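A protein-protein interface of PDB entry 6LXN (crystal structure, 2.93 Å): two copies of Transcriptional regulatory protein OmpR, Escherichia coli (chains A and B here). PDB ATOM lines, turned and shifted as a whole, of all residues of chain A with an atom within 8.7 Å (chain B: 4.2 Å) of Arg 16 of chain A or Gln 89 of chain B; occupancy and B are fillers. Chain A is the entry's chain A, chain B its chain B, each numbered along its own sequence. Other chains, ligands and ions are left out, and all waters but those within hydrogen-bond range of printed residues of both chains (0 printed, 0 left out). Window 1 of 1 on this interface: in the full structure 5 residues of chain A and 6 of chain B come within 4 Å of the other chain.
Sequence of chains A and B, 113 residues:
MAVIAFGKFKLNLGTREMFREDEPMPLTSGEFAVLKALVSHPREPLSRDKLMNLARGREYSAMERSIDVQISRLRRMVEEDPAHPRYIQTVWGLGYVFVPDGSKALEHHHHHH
The backbone carbonyl oxygen (O) of Thr 15 of chain A sits at hydrogen-bond distance from the side-chain amide nitrogen (NE2) of Gln 89 of chain B (3.0 Å).
The guanidinium group (NH2) of Arg 16 of chain A is in hydrogen-bond range of the backbone carbonyl oxygen (O) of Thr 90 of chain B (2.9 Å).
OG of Ser 29 of chain A is in hydrogen-bond range of O of Thr 90 of chain B (3.2 Å).
The guanidinium group (NE) of Arg 16 of chain A sits at hydrogen-bond distance from the side-chain amide oxygen (OE1) of Gln 89 of chain B, 2.9 Å away.
The side-chain carboxylate of Glu 17 of chain A lies within salt-bridge range of the guanidinium group of Arg 86 of chain B (3.7 Å).
The backbone carbonyl oxygen of Val 97 of chain B is in hydrogen-bond range of the backbone NH of Gln 89 of chain B.
NH1 of Arg 16 of chain A sits at hydrogen-bond distance from OG of Ser 29 of chain A (3.1 Å).
O of Arg 86 of chain B lies within hydrogen-bond range of NE2 of Gln 89 of chain B, at 3.3 Å.
The guanidinium group (NH1) of Arg 86 of chain B sits at hydrogen-bond distance from the backbone carbonyl oxygen (O) of Val 99 of chain B (2.8 Å).
The side-chain amide oxygen (OD1) of Asn 12 of chain A sits at hydrogen-bond distance from the backbone NH (N) of Thr 15 of chain A, 3.1 Å away.
O of Glu 17 of chain A sits at hydrogen-bond distance from N of Asn 12 of chain A (2.9 Å).
Among the printed residues, pairs that only touch across the chains: Thr 15 of chain A with Arg 86 of chain B.
Arg 16 of chain A touches just these residues of chain B: Gln 89 (2.9 Å) and Thr 90 (2.9 Å).
Gln 89 of chain B touches just these residues of chain A: Thr 15 (3.0 Å) and Arg 16 (2.9 Å).
Of the printed residues of chain B, Thr 15 of chain A touches Arg 86 and Gln 89.
Printed residues of chain A within 4 Å of Arg 86 of chain B: Thr 15 (3.4 Å) and Glu 17 (3.7 Å).
Of the printed residues of chain A, Thr 90 of chain B touches Arg 16 (2.9 Å) and Ser 29 (3.2 Å).
Printed residues of chain B within 4 Å of Ser 29 of chain A: Thr 90 (3.2 Å).
Ala 2 of chain A touches none of the printed residues of chain B.
The nearest printed residue of chain B that does not touch Arg 16 of chain A is Val 97 of chain B (5.1 Å).
The nearest residue of chain A that does not touch Gln 89 of chain B is Glu 17 of chain A (5.6 Å).
Printed residues of chain A that touch a printed residue of chain B: Thr 15, Arg 16, Glu 17 and Ser 29.
Of the 10 printed residues of chain B, 3 touch a printed residue of chain A.
No position is printed for both chains.
Of the 6 pairs that touch across the chains among the printed residues, none has its exchanged pair printed and touching as well.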
ATOM      1  N   ALA A   2     -13.554  -6.278  22.204  1.00  0.00           N
ATOM      2  CA  ALA A   2     -14.854  -5.972  21.623  1.00  0.00           C
ATOM      3  C   ALA A   2     -15.569  -7.250  21.189  1.00  0.00           C
ATOM      4  O   ALA A   2     -15.563  -8.250  21.911  1.00  0.00           O
ATOM      5  CB  ALA A   2     -14.704  -5.008  20.437  1.00  0.00           C
ATOM      6  N   LYS A  10     -22.062 -14.167  17.535  1.00  0.00           N
ATOM      7  CA  LYS A  10     -21.260 -13.011  17.892  1.00  0.00           C
ATOM      8  C   LYS A  10     -21.177 -12.981  19.416  1.00  0.00           C
ATOM      9  O   LYS A  10     -22.152 -13.296  20.104  1.00  0.00           O
ATOM     10  CB  LYS A  10     -21.848 -11.708  17.329  1.00  0.00           C
ATOM     11  CG  LYS A  10     -22.579 -11.871  15.980  1.00  0.00           C
ATOM     12  CD  LYS A  10     -23.195 -10.531  15.472  1.00  0.00           C
ATOM     13  CE  LYS A  10     -23.795 -10.620  14.050  1.00  0.00           C
ATOM     14  NZ  LYS A  10     -24.471 -11.930  13.814  1.00  0.00           N
ATOM     15  N   LEU A  11     -19.995 -12.656  19.939  1.00  0.00           N
ATOM     16  CA  LEU A  11     -19.728 -12.739  21.372  1.00  0.00           C
ATOM     17  C   LEU A  11     -18.981 -11.488  21.810  1.00  0.00           C
ATOM     18  O   LEU A  11     -17.903 -11.179  21.281  1.00  0.00           O
ATOM     19  CB  LEU A  11     -18.911 -13.992  21.710  1.00  0.00           C
ATOM     20  CG  LEU A  11     -18.270 -14.059  23.107  1.00  0.00           C
ATOM     21  CD1 LEU A  11     -19.302 -14.303  24.189  1.00  0.00           C
ATOM     22  CD2 LEU A  11     -17.194 -15.118  23.146  1.00  0.00           C
ATOM     23  N   ASN A  12     -19.543 -10.789  22.796  1.00  0.00           N
ATOM     24  CA  ASN A  12     -19.009  -9.515  23.276  1.00  0.00           C
ATOM     25  C   ASN A  12     -18.118  -9.774  24.484  1.00  0.00           C
ATOM     26  O   ASN A  12     -18.590  -9.863  25.620  1.00  0.00           O
ATOM     27  CB  ASN A  12     -20.150  -8.566  23.625  1.00  0.00           C
ATOM     28  CG  ASN A  12     -19.690  -7.136  23.784  1.00  0.00           C
ATOM     29  OD1 ASN A  12     -18.799  -6.830  24.584  1.00  0.00           O
ATOM     30  ND2 ASN A  12     -20.297  -6.244  23.018  1.00  0.00           N
ATOM     31  N   LEU A  13     -16.807  -9.860  24.247  1.00  0.00           N
ATOM     32  CA  LEU A  13     -15.856 -10.041  25.346  1.00  0.00           C
ATOM     33  C   LEU A  13     -16.006  -8.967  26.423  1.00  0.00           C
ATOM     34  O   LEU A  13     -15.693  -9.211  27.591  1.00  0.00           O
ATOM     35  CB  LEU A  13     -14.419 -10.042  24.803  1.00  0.00           C
ATOM     36  CG  LEU A  13     -13.761 -11.295  24.185  1.00  0.00           C
ATOM     37  CD1 LEU A  13     -14.696 -12.109  23.289  1.00  0.00           C
ATOM     38  CD2 LEU A  13     -12.504 -10.917  23.394  1.00  0.00           C
ATOM     39  N   GLY A  14     -16.489  -7.778  26.060  1.00  0.00           N
ATOM     40  CA  GLY A  14     -16.597  -6.707  27.042  1.00  0.00           C
ATOM     41  C   GLY A  14     -17.689  -6.944  28.066  1.00  0.00           C
ATOM     42  O   GLY A  14     -17.492  -6.723  29.261  1.00  0.00           O
ATOM     43  N   THR A  15     -18.847  -7.419  27.618  1.00  0.00           N
ATOM     44  CA  THR A  15     -20.021  -7.528  28.475  1.00  0.00           C
ATOM     45  C   THR A  15     -20.458  -8.960  28.761  1.00  0.00           C
ATOM     46  O   THR A  15     -21.369  -9.160  29.574  1.00  0.00           O
ATOM     47  CB  THR A  15     -21.188  -6.766  27.836  1.00  0.00           C
ATOM     48  OG1 THR A  15     -21.373  -7.247  26.504  1.00  0.00           O
ATOM     49  CG2 THR A  15     -20.862  -5.309  27.754  1.00  0.00           C
ATOM     50  N   ARG A  16     -19.835  -9.952  28.129  1.00  0.00           N
ATOM     51  CA  ARG A  16     -20.241 -11.357  28.192  1.00  0.00           C
ATOM     52  C   ARG A  16     -21.599 -11.603  27.546  1.00  0.00           C
ATOM     53  O   ARG A  16     -22.234 -12.634  27.805  1.00  0.00           O
ATOM     54  CB  ARG A  16     -20.236 -11.899  29.626  1.00  0.00           C
ATOM     55  CG  ARG A  16     -19.054 -11.425  30.397  1.00  0.00           C
ATOM     56  CD  ARG A  16     -18.875 -12.143  31.695  1.00  0.00           C
ATOM     57  NE  ARG A  16     -19.915 -11.836  32.661  1.00  0.00           N
ATOM     58  CZ  ARG A  16     -20.015 -12.458  33.826  1.00  0.00           C
ATOM     59  NH1 ARG A  16     -19.126 -13.402  34.142  1.00  0.00           N
ATOM     60  NH2 ARG A  16     -20.993 -12.148  34.667  1.00  0.00           N
ATOM     61  N   GLU A  17     -22.069 -10.697  26.698  1.00  0.00           N
ATOM     62  CA  GLU A  17     -23.267 -11.005  25.938  1.00  0.00           C
ATOM     63  C   GLU A  17     -22.907 -11.895  24.757  1.00  0.00           C
ATOM     64  O   GLU A  17     -21.794 -11.835  24.223  1.00  0.00           O
ATOM     65  CB  GLU A  17     -23.954  -9.732  25.439  1.00  0.00           C
ATOM     66  CG  GLU A  17     -24.169  -8.672  26.506  1.00  0.00           C
ATOM     67  CD  GLU A  17     -25.116  -7.580  26.050  1.00  0.00           C
ATOM     68  OE1 GLU A  17     -24.638  -6.450  25.790  1.00  0.00           O
ATOM     69  OE2 GLU A  17     -26.336  -7.856  25.960  1.00  0.00           O
ATOM     70  N   MET A  18     -23.860 -12.732  24.355  1.00  0.00           N
ATOM     71  CA  MET A  18     -23.671 -13.565  23.177  1.00  0.00           C
ATOM     72  C   MET A  18     -24.990 -13.682  22.426  1.00  0.00           C
ATOM     73  O   MET A  18     -26.066 -13.711  23.035  1.00  0.00           O
ATOM     74  CB  MET A  18     -23.132 -14.953  23.542  1.00  0.00           C
ATOM     75  CG  MET A  18     -23.358 -15.983  22.461  1.00  0.00           C
ATOM     76  SD  MET A  18     -22.192 -17.349  22.452  1.00  0.00           S
ATOM     77  CE  MET A  18     -21.024 -16.775  21.231  1.00  0.00           C
ATOM     78  N   PHE A  19     -24.891 -13.733  21.095  1.00  0.00           N
ATOM     79  CA  PHE A  19     -26.039 -13.782  20.204  1.00  0.00           C
ATOM     80  C   PHE A  19     -25.779 -14.774  19.084  1.00  0.00           C
ATOM     81  O   PHE A  19     -24.692 -14.786  18.499  1.00  0.00           O
ATOM     82  CB  PHE A  19     -26.334 -12.418  19.574  1.00  0.00           C
ATOM     83  CG  PHE A  19     -26.282 -11.269  20.540  1.00  0.00           C
ATOM     84  CD1 PHE A  19     -25.061 -10.741  20.945  1.00  0.00           C
ATOM     85  CD2 PHE A  19     -27.457 -10.697  21.021  1.00  0.00           C
ATOM     86  CE1 PHE A  19     -25.010  -9.688  21.832  1.00  0.00           C
ATOM     87  CE2 PHE A  19     -27.415  -9.639  21.902  1.00  0.00           C
ATOM     88  CZ  PHE A  19     -26.187  -9.130  22.310  1.00  0.00           C
ATOM     89  N   MET A  25     -28.335 -15.107  23.661  1.00  0.00           N
ATOM     90  CA  MET A  25     -28.247 -16.405  24.327  1.00  0.00           C
ATOM     91  C   MET A  25     -27.308 -16.315  25.531  1.00  0.00           C
ATOM     92  O   MET A  25     -26.125 -15.979  25.393  1.00  0.00           O
ATOM     93  CB  MET A  25     -27.820 -17.508  23.347  1.00  0.00           C
ATOM     94  CG  MET A  25     -26.344 -17.612  23.031  1.00  0.00           C
ATOM     95  SD  MET A  25     -25.957 -18.981  21.914  1.00  0.00           S
ATOM     96  CE  MET A  25     -27.376 -20.064  22.139  1.00  0.00           C
ATOM     97  N   PRO A  26     -27.819 -16.562  26.732  1.00  0.00           N
ATOM     98  CA  PRO A  26     -27.000 -16.388  27.930  1.00  0.00           C
ATOM     99  C   PRO A  26     -25.859 -17.382  28.015  1.00  0.00           C
ATOM    100  O   PRO A  26     -25.958 -18.532  27.585  1.00  0.00           O
ATOM    101  CB  PRO A  26     -27.997 -16.611  29.074  1.00  0.00           C
ATOM    102  CG  PRO A  26     -29.273 -16.201  28.505  1.00  0.00           C
ATOM    103  CD  PRO A  26     -29.232 -16.726  27.088  1.00  0.00           C
ATOM    104  N   LEU A  27     -24.765 -16.904  28.594  1.00  0.00           N
ATOM    105  CA  LEU A  27     -23.640 -17.728  28.985  1.00  0.00           C
ATOM    106  C   LEU A  27     -23.509 -17.644  30.496  1.00  0.00           C
ATOM    107  O   LEU A  27     -23.621 -16.565  31.076  1.00  0.00           O
ATOM    108  CB  LEU A  27     -22.347 -17.262  28.305  1.00  0.00           C
ATOM    109  CG  LEU A  27     -22.310 -17.452  26.781  1.00  0.00           C
ATOM    110  CD1 LEU A  27     -21.312 -16.527  26.138  1.00  0.00           C
ATOM    111  CD2 LEU A  27     -21.989 -18.892  26.426  1.00  0.00           C
ATOM    112  N   THR A  28     -23.304 -18.780  31.133  1.00  0.00           N
ATOM    113  CA  THR A  28     -22.936 -18.748  32.532  1.00  0.00           C
ATOM    114  C   THR A  28     -21.539 -18.159  32.680  1.00  0.00           C
ATOM    115  O   THR A  28     -20.773 -18.064  31.719  1.00  0.00           O
ATOM    116  CB  THR A  28     -22.964 -20.154  33.112  1.00  0.00           C
ATOM    117  OG1 THR A  28     -21.816 -20.865  32.641  1.00  0.00           O
ATOM    118  CG2 THR A  28     -24.173 -20.865  32.614  1.00  0.00           C
ATOM    119  N   SER A  29     -21.188 -17.801  33.915  1.00  0.00           N
ATOM    120  CA  SER A  29     -19.886 -17.184  34.133  1.00  0.00           C
ATOM    121  C   SER A  29     -18.764 -18.133  33.747  1.00  0.00           C
ATOM    122  O   SER A  29     -17.835 -17.759  33.024  1.00  0.00           O
ATOM    123  CB  SER A  29     -19.764 -16.724  35.578  1.00  0.00           C
ATOM    124  OG  SER A  29     -20.580 -15.578  35.779  1.00  0.00           O
ATOM    125  N   GLY A  30     -18.867 -19.383  34.172  1.00  0.00           N
ATOM    126  CA  GLY A  30     -17.879 -20.365  33.781  1.00  0.00           C
ATOM    127  C   GLY A  30     -17.796 -20.576  32.283  1.00  0.00           C
ATOM    128  O   GLY A  30     -16.714 -20.829  31.749  1.00  0.00           O
ATOM    129  N   GLU A  31     -18.925 -20.460  31.583  1.00  0.00           N
ATOM    130  CA  GLU A  31     -18.889 -20.659  30.137  1.00  0.00           C
ATOM    131  C   GLU A  31     -18.238 -19.482  29.432  1.00  0.00           C
ATOM    132  O   GLU A  31     -17.465 -19.671  28.491  1.00  0.00           O
ATOM    133  CB  GLU A  31     -20.290 -20.897  29.602  1.00  0.00           C
ATOM    134  CG  GLU A  31     -20.867 -22.185  30.087  1.00  0.00           C
ATOM    135  CD  GLU A  31     -22.350 -22.211  29.942  1.00  0.00           C
ATOM    136  OE1 GLU A  31     -22.910 -21.129  29.649  1.00  0.00           O
ATOM    137  OE2 GLU A  31     -22.947 -23.298  30.129  1.00  0.00           O
ATOM    138  N   PHE A  32     -18.522 -18.263  29.871  1.00  0.00           N
ATOM    139  CA  PHE A  32     -17.836 -17.122  29.279  1.00  0.00           C
ATOM    140  C   PHE A  32     -16.345 -17.236  29.478  1.00  0.00           C
ATOM    141  O   PHE A  32     -15.568 -17.050  28.534  1.00  0.00           O
ATOM    142  CB  PHE A  32     -18.314 -15.822  29.896  1.00  0.00           C
ATOM    143  CG  PHE A  32     -17.592 -14.635  29.377  1.00  0.00           C
ATOM    144  CD1 PHE A  32     -17.866 -14.147  28.124  1.00  0.00           C
ATOM    145  CD2 PHE A  32     -16.633 -14.014  30.133  1.00  0.00           C
ATOM    146  CE1 PHE A  32     -17.193 -13.053  27.635  1.00  0.00           C
ATOM    147  CE2 PHE A  32     -15.974 -12.913  29.652  1.00  0.00           C
ATOM    148  CZ  PHE A  32     -16.254 -12.441  28.396  1.00  0.00           C
ATOM    149  N   ALA A  33     -15.934 -17.557  30.702  1.00  0.00           N
ATOM    150  CA  ALA A  33     -14.520 -17.618  31.030  1.00  0.00           C
ATOM    151  C   ALA A  33     -13.753 -18.486  30.038  1.00  0.00           C
ATOM    152  O   ALA A  33     -12.865 -17.994  29.327  1.00  0.00           O
ATOM    153  CB  ALA A  33     -14.349 -18.114  32.456  1.00  0.00           C
ATOM    154  N   LEU A  35     -14.756 -19.887  27.323  1.00  0.00           N
ATOM    155  CA  LEU A  35     -15.009 -19.492  25.943  1.00  0.00           C
ATOM    156  C   LEU A  35     -14.127 -18.316  25.553  1.00  0.00           C
ATOM    157  O   LEU A  35     -13.458 -18.361  24.516  1.00  0.00           O
ATOM    158  CB  LEU A  35     -16.480 -19.163  25.718  1.00  0.00           C
ATOM    159  CG  LEU A  35     -16.820 -18.817  24.272  1.00  0.00           C
ATOM    160  CD1 LEU A  35     -16.806 -20.077  23.436  1.00  0.00           C
ATOM    161  CD2 LEU A  35     -18.189 -18.174  24.222  1.00  0.00           C
ATOM    162  N   LYS A  36     -14.073 -17.274  26.399  1.00  0.00           N
ATOM    163  CA  LYS A  36     -13.243 -16.108  26.073  1.00  0.00           C
ATOM    164  C   LYS A  36     -11.784 -16.498  25.853  1.00  0.00           C
ATOM    165  O   LYS A  36     -11.202 -16.160  24.818  1.00  0.00           O
ATOM    166  CB  LYS A  36     -13.333 -15.030  27.157  1.00  0.00           C
ATOM    167  CG  LYS A  36     -12.216 -13.958  27.030  1.00  0.00           C
ATOM    168  CD  LYS A  36     -12.399 -12.821  28.072  1.00  0.00           C
ATOM    169  CE  LYS A  36     -11.223 -12.689  29.063  1.00  0.00           C
ATOM    170  NZ  LYS A  36     -11.673 -12.153  30.405  1.00  0.00           N
ATOM    171  N   ARG B  75     -31.349  -4.687  40.783  1.00  0.00           N
ATOM    172  CA  ARG B  75     -31.707  -5.078  39.416  1.00  0.00           C
ATOM    173  C   ARG B  75     -33.174  -4.796  39.118  1.00  0.00           C
ATOM    174  O   ARG B  75     -33.504  -4.238  38.062  1.00  0.00           O
ATOM    175  CB  ARG B  75     -31.419  -6.556  39.178  1.00  0.00           C
ATOM    176  CG  ARG B  75     -30.015  -6.870  38.756  1.00  0.00           C
ATOM    177  CD  ARG B  75     -29.470  -7.968  39.641  1.00  0.00           C
ATOM    178  NE  ARG B  75     -28.310  -8.651  39.086  1.00  0.00           N
ATOM    179  CZ  ARG B  75     -27.889  -9.826  39.531  1.00  0.00           C
ATOM    180  NH1 ARG B  75     -28.545 -10.433  40.527  1.00  0.00           N
ATOM    181  NH2 ARG B  75     -26.824 -10.392  38.984  1.00  0.00           N
ATOM    182  N   PRO B  85     -29.343  -9.803  33.523  1.00  0.00           N
ATOM    183  CA  PRO B  85     -28.873  -8.430  33.766  1.00  0.00           C
ATOM    184  C   PRO B  85     -27.609  -8.064  33.010  1.00  0.00           C
ATOM    185  O   PRO B  85     -26.686  -8.869  32.852  1.00  0.00           O
ATOM    186  CB  PRO B  85     -28.621  -8.407  35.280  1.00  0.00           C
ATOM    187  CG  PRO B  85     -28.443  -9.846  35.668  1.00  0.00           C
ATOM    188  CD  PRO B  85     -29.282 -10.645  34.730  1.00  0.00           C
ATOM    189  N   ARG B  86     -27.578  -6.807  32.566  1.00  0.00           N
ATOM    190  CA  ARG B  86     -26.470  -6.265  31.794  1.00  0.00           C
ATOM    191  C   ARG B  86     -25.554  -5.350  32.592  1.00  0.00           C
ATOM    192  O   ARG B  86     -24.342  -5.418  32.424  1.00  0.00           O
ATOM    193  CB  ARG B  86     -26.986  -5.490  30.574  1.00  0.00           C
ATOM    194  CG  ARG B  86     -26.052  -4.384  30.115  1.00  0.00           C
ATOM    195  CD  ARG B  86     -25.019  -4.980  29.149  1.00  0.00           C
ATOM    196  NE  ARG B  86     -24.218  -3.979  28.452  1.00  0.00           N
ATOM    197  CZ  ARG B  86     -23.226  -3.275  29.000  1.00  0.00           C
ATOM    198  NH1 ARG B  86     -22.896  -3.426  30.278  1.00  0.00           N
ATOM    199  NH2 ARG B  86     -22.557  -2.402  28.256  1.00  0.00           N
ATOM    200  N   TYR B  87     -26.076  -4.475  33.451  1.00  0.00           N
ATOM    201  CA  TYR B  87     -25.167  -3.566  34.140  1.00  0.00           C
ATOM    202  C   TYR B  87     -24.684  -4.128  35.474  1.00  0.00           C
ATOM    203  O   TYR B  87     -23.506  -3.981  35.804  1.00  0.00           O
ATOM    204  CB  TYR B  87     -25.838  -2.196  34.302  1.00  0.00           C
ATOM    205  CG  TYR B  87     -26.217  -1.578  32.962  1.00  0.00           C
ATOM    206  CD1 TYR B  87     -25.251  -0.973  32.154  1.00  0.00           C
ATOM    207  CD2 TYR B  87     -27.513  -1.658  32.475  1.00  0.00           C
ATOM    208  CE1 TYR B  87     -25.578  -0.437  30.911  1.00  0.00           C
ATOM    209  CE2 TYR B  87     -27.852  -1.119  31.238  1.00  0.00           C
ATOM    210  CZ  TYR B  87     -26.884  -0.508  30.456  1.00  0.00           C
ATOM    211  OH  TYR B  87     -27.230   0.026  29.217  1.00  0.00           O
ATOM    212  N   ILE B  88     -25.548  -4.801  36.239  1.00  0.00           N
ATOM    213  CA  ILE B  88     -25.131  -5.404  37.504  1.00  0.00           C
ATOM    214  C   ILE B  88     -25.102  -6.918  37.366  1.00  0.00           C
ATOM    215  O   ILE B  88     -26.107  -7.604  37.583  1.00  0.00           O
ATOM    216  CB  ILE B  88     -26.044  -4.974  38.660  1.00  0.00           C
ATOM    217  CG1 ILE B  88     -25.968  -3.462  38.839  1.00  0.00           C
ATOM    218  CG2 ILE B  88     -25.627  -5.677  39.948  1.00  0.00           C
ATOM    219  CD1 ILE B  88     -27.260  -2.847  39.356  1.00  0.00           C
ATOM    220  N   GLN B  89     -23.955  -7.448  36.993  1.00  0.00           N
ATOM    221  CA  GLN B  89     -23.891  -8.863  36.687  1.00  0.00           C
ATOM    222  C   GLN B  89     -23.404  -9.655  37.882  1.00  0.00           C
ATOM    223  O   GLN B  89     -22.836  -9.113  38.833  1.00  0.00           O
ATOM    224  CB  GLN B  89     -22.995  -9.160  35.478  1.00  0.00           C
ATOM    225  CG  GLN B  89     -23.042  -8.141  34.358  1.00  0.00           C
ATOM    226  CD  GLN B  89     -22.452  -8.729  33.086  1.00  0.00           C
ATOM    227  OE1 GLN B  89     -21.497  -9.511  33.132  1.00  0.00           O
ATOM    228  NE2 GLN B  89     -23.000  -8.341  31.946  1.00  0.00           N
ATOM    229  N   THR B  90     -23.634 -10.963  37.823  1.00  0.00           N
ATOM    230  CA  THR B  90     -23.172 -11.862  38.864  1.00  0.00           C
ATOM    231  C   THR B  90     -22.046 -12.735  38.329  1.00  0.00           C
ATOM    232  O   THR B  90     -22.089 -13.192  37.182  1.00  0.00           O
ATOM    233  CB  THR B  90     -24.307 -12.711  39.423  1.00  0.00           C
ATOM    234  OG1 THR B  90     -23.732 -13.782  40.178  1.00  0.00           O
ATOM    235  CG2 THR B  90     -25.199 -13.264  38.319  1.00  0.00           C
ATOM    236  N   TYR B  96     -20.198  -9.838  42.612  1.00  0.00           N
ATOM    237  CA  TYR B  96     -20.909  -9.089  41.587  1.00  0.00           C
ATOM    238  C   TYR B  96     -19.955  -8.087  40.948  1.00  0.00           C
ATOM    239  O   TYR B  96     -18.925  -7.731  41.524  1.00  0.00           O
ATOM    240  CB  TYR B  96     -22.117  -8.377  42.194  1.00  0.00           C
ATOM    241  CG  TYR B  96     -23.006  -9.335  42.912  1.00  0.00           C
ATOM    242  CD1 TYR B  96     -22.754  -9.692  44.238  1.00  0.00           C
ATOM    243  CD2 TYR B  96     -24.095  -9.917  42.261  1.00  0.00           C
ATOM    244  CE1 TYR B  96     -23.572 -10.619  44.901  1.00  0.00           C
ATOM    245  CE2 TYR B  96     -24.920 -10.833  42.911  1.00  0.00           C
ATOM    246  CZ  TYR B  96     -24.648 -11.186  44.227  1.00  0.00           C
ATOM    247  OH  TYR B  96     -25.457 -12.101  44.855  1.00  0.00           O
ATOM    248  N   VAL B  97     -20.289  -7.635  39.742  1.00  0.00           N
ATOM    249  CA  VAL B  97     -19.484  -6.633  39.058  1.00  0.00           C
ATOM    250  C   VAL B  97     -20.393  -5.727  38.241  1.00  0.00           C
ATOM    251  O   VAL B  97     -21.448  -6.145  37.750  1.00  0.00           O
ATOM    252  CB  VAL B  97     -18.406  -7.285  38.169  1.00  0.00           C
ATOM    253  CG1 VAL B  97     -19.059  -8.079  37.045  1.00  0.00           C
ATOM    254  CG2 VAL B  97     -17.432  -6.230  37.623  1.00  0.00           C
ATOM    255  N   VAL B  99     -20.477  -3.788  34.866  1.00  0.00           N
ATOM    256  CA  VAL B  99     -19.827  -3.655  33.558  1.00  0.00           C
ATOM    257  C   VAL B  99     -20.429  -2.422  32.887  1.00  0.00           C
ATOM    258  O   VAL B  99     -21.627  -2.429  32.553  1.00  0.00           O
ATOM    259  CB  VAL B  99     -19.947  -4.922  32.701  1.00  0.00           C
ATOM    260  CG1 VAL B  99     -19.123  -6.028  33.321  1.00  0.00           C
ATOM    261  CG2 VAL B  99     -21.360  -5.390  32.601  1.00  0.00           C
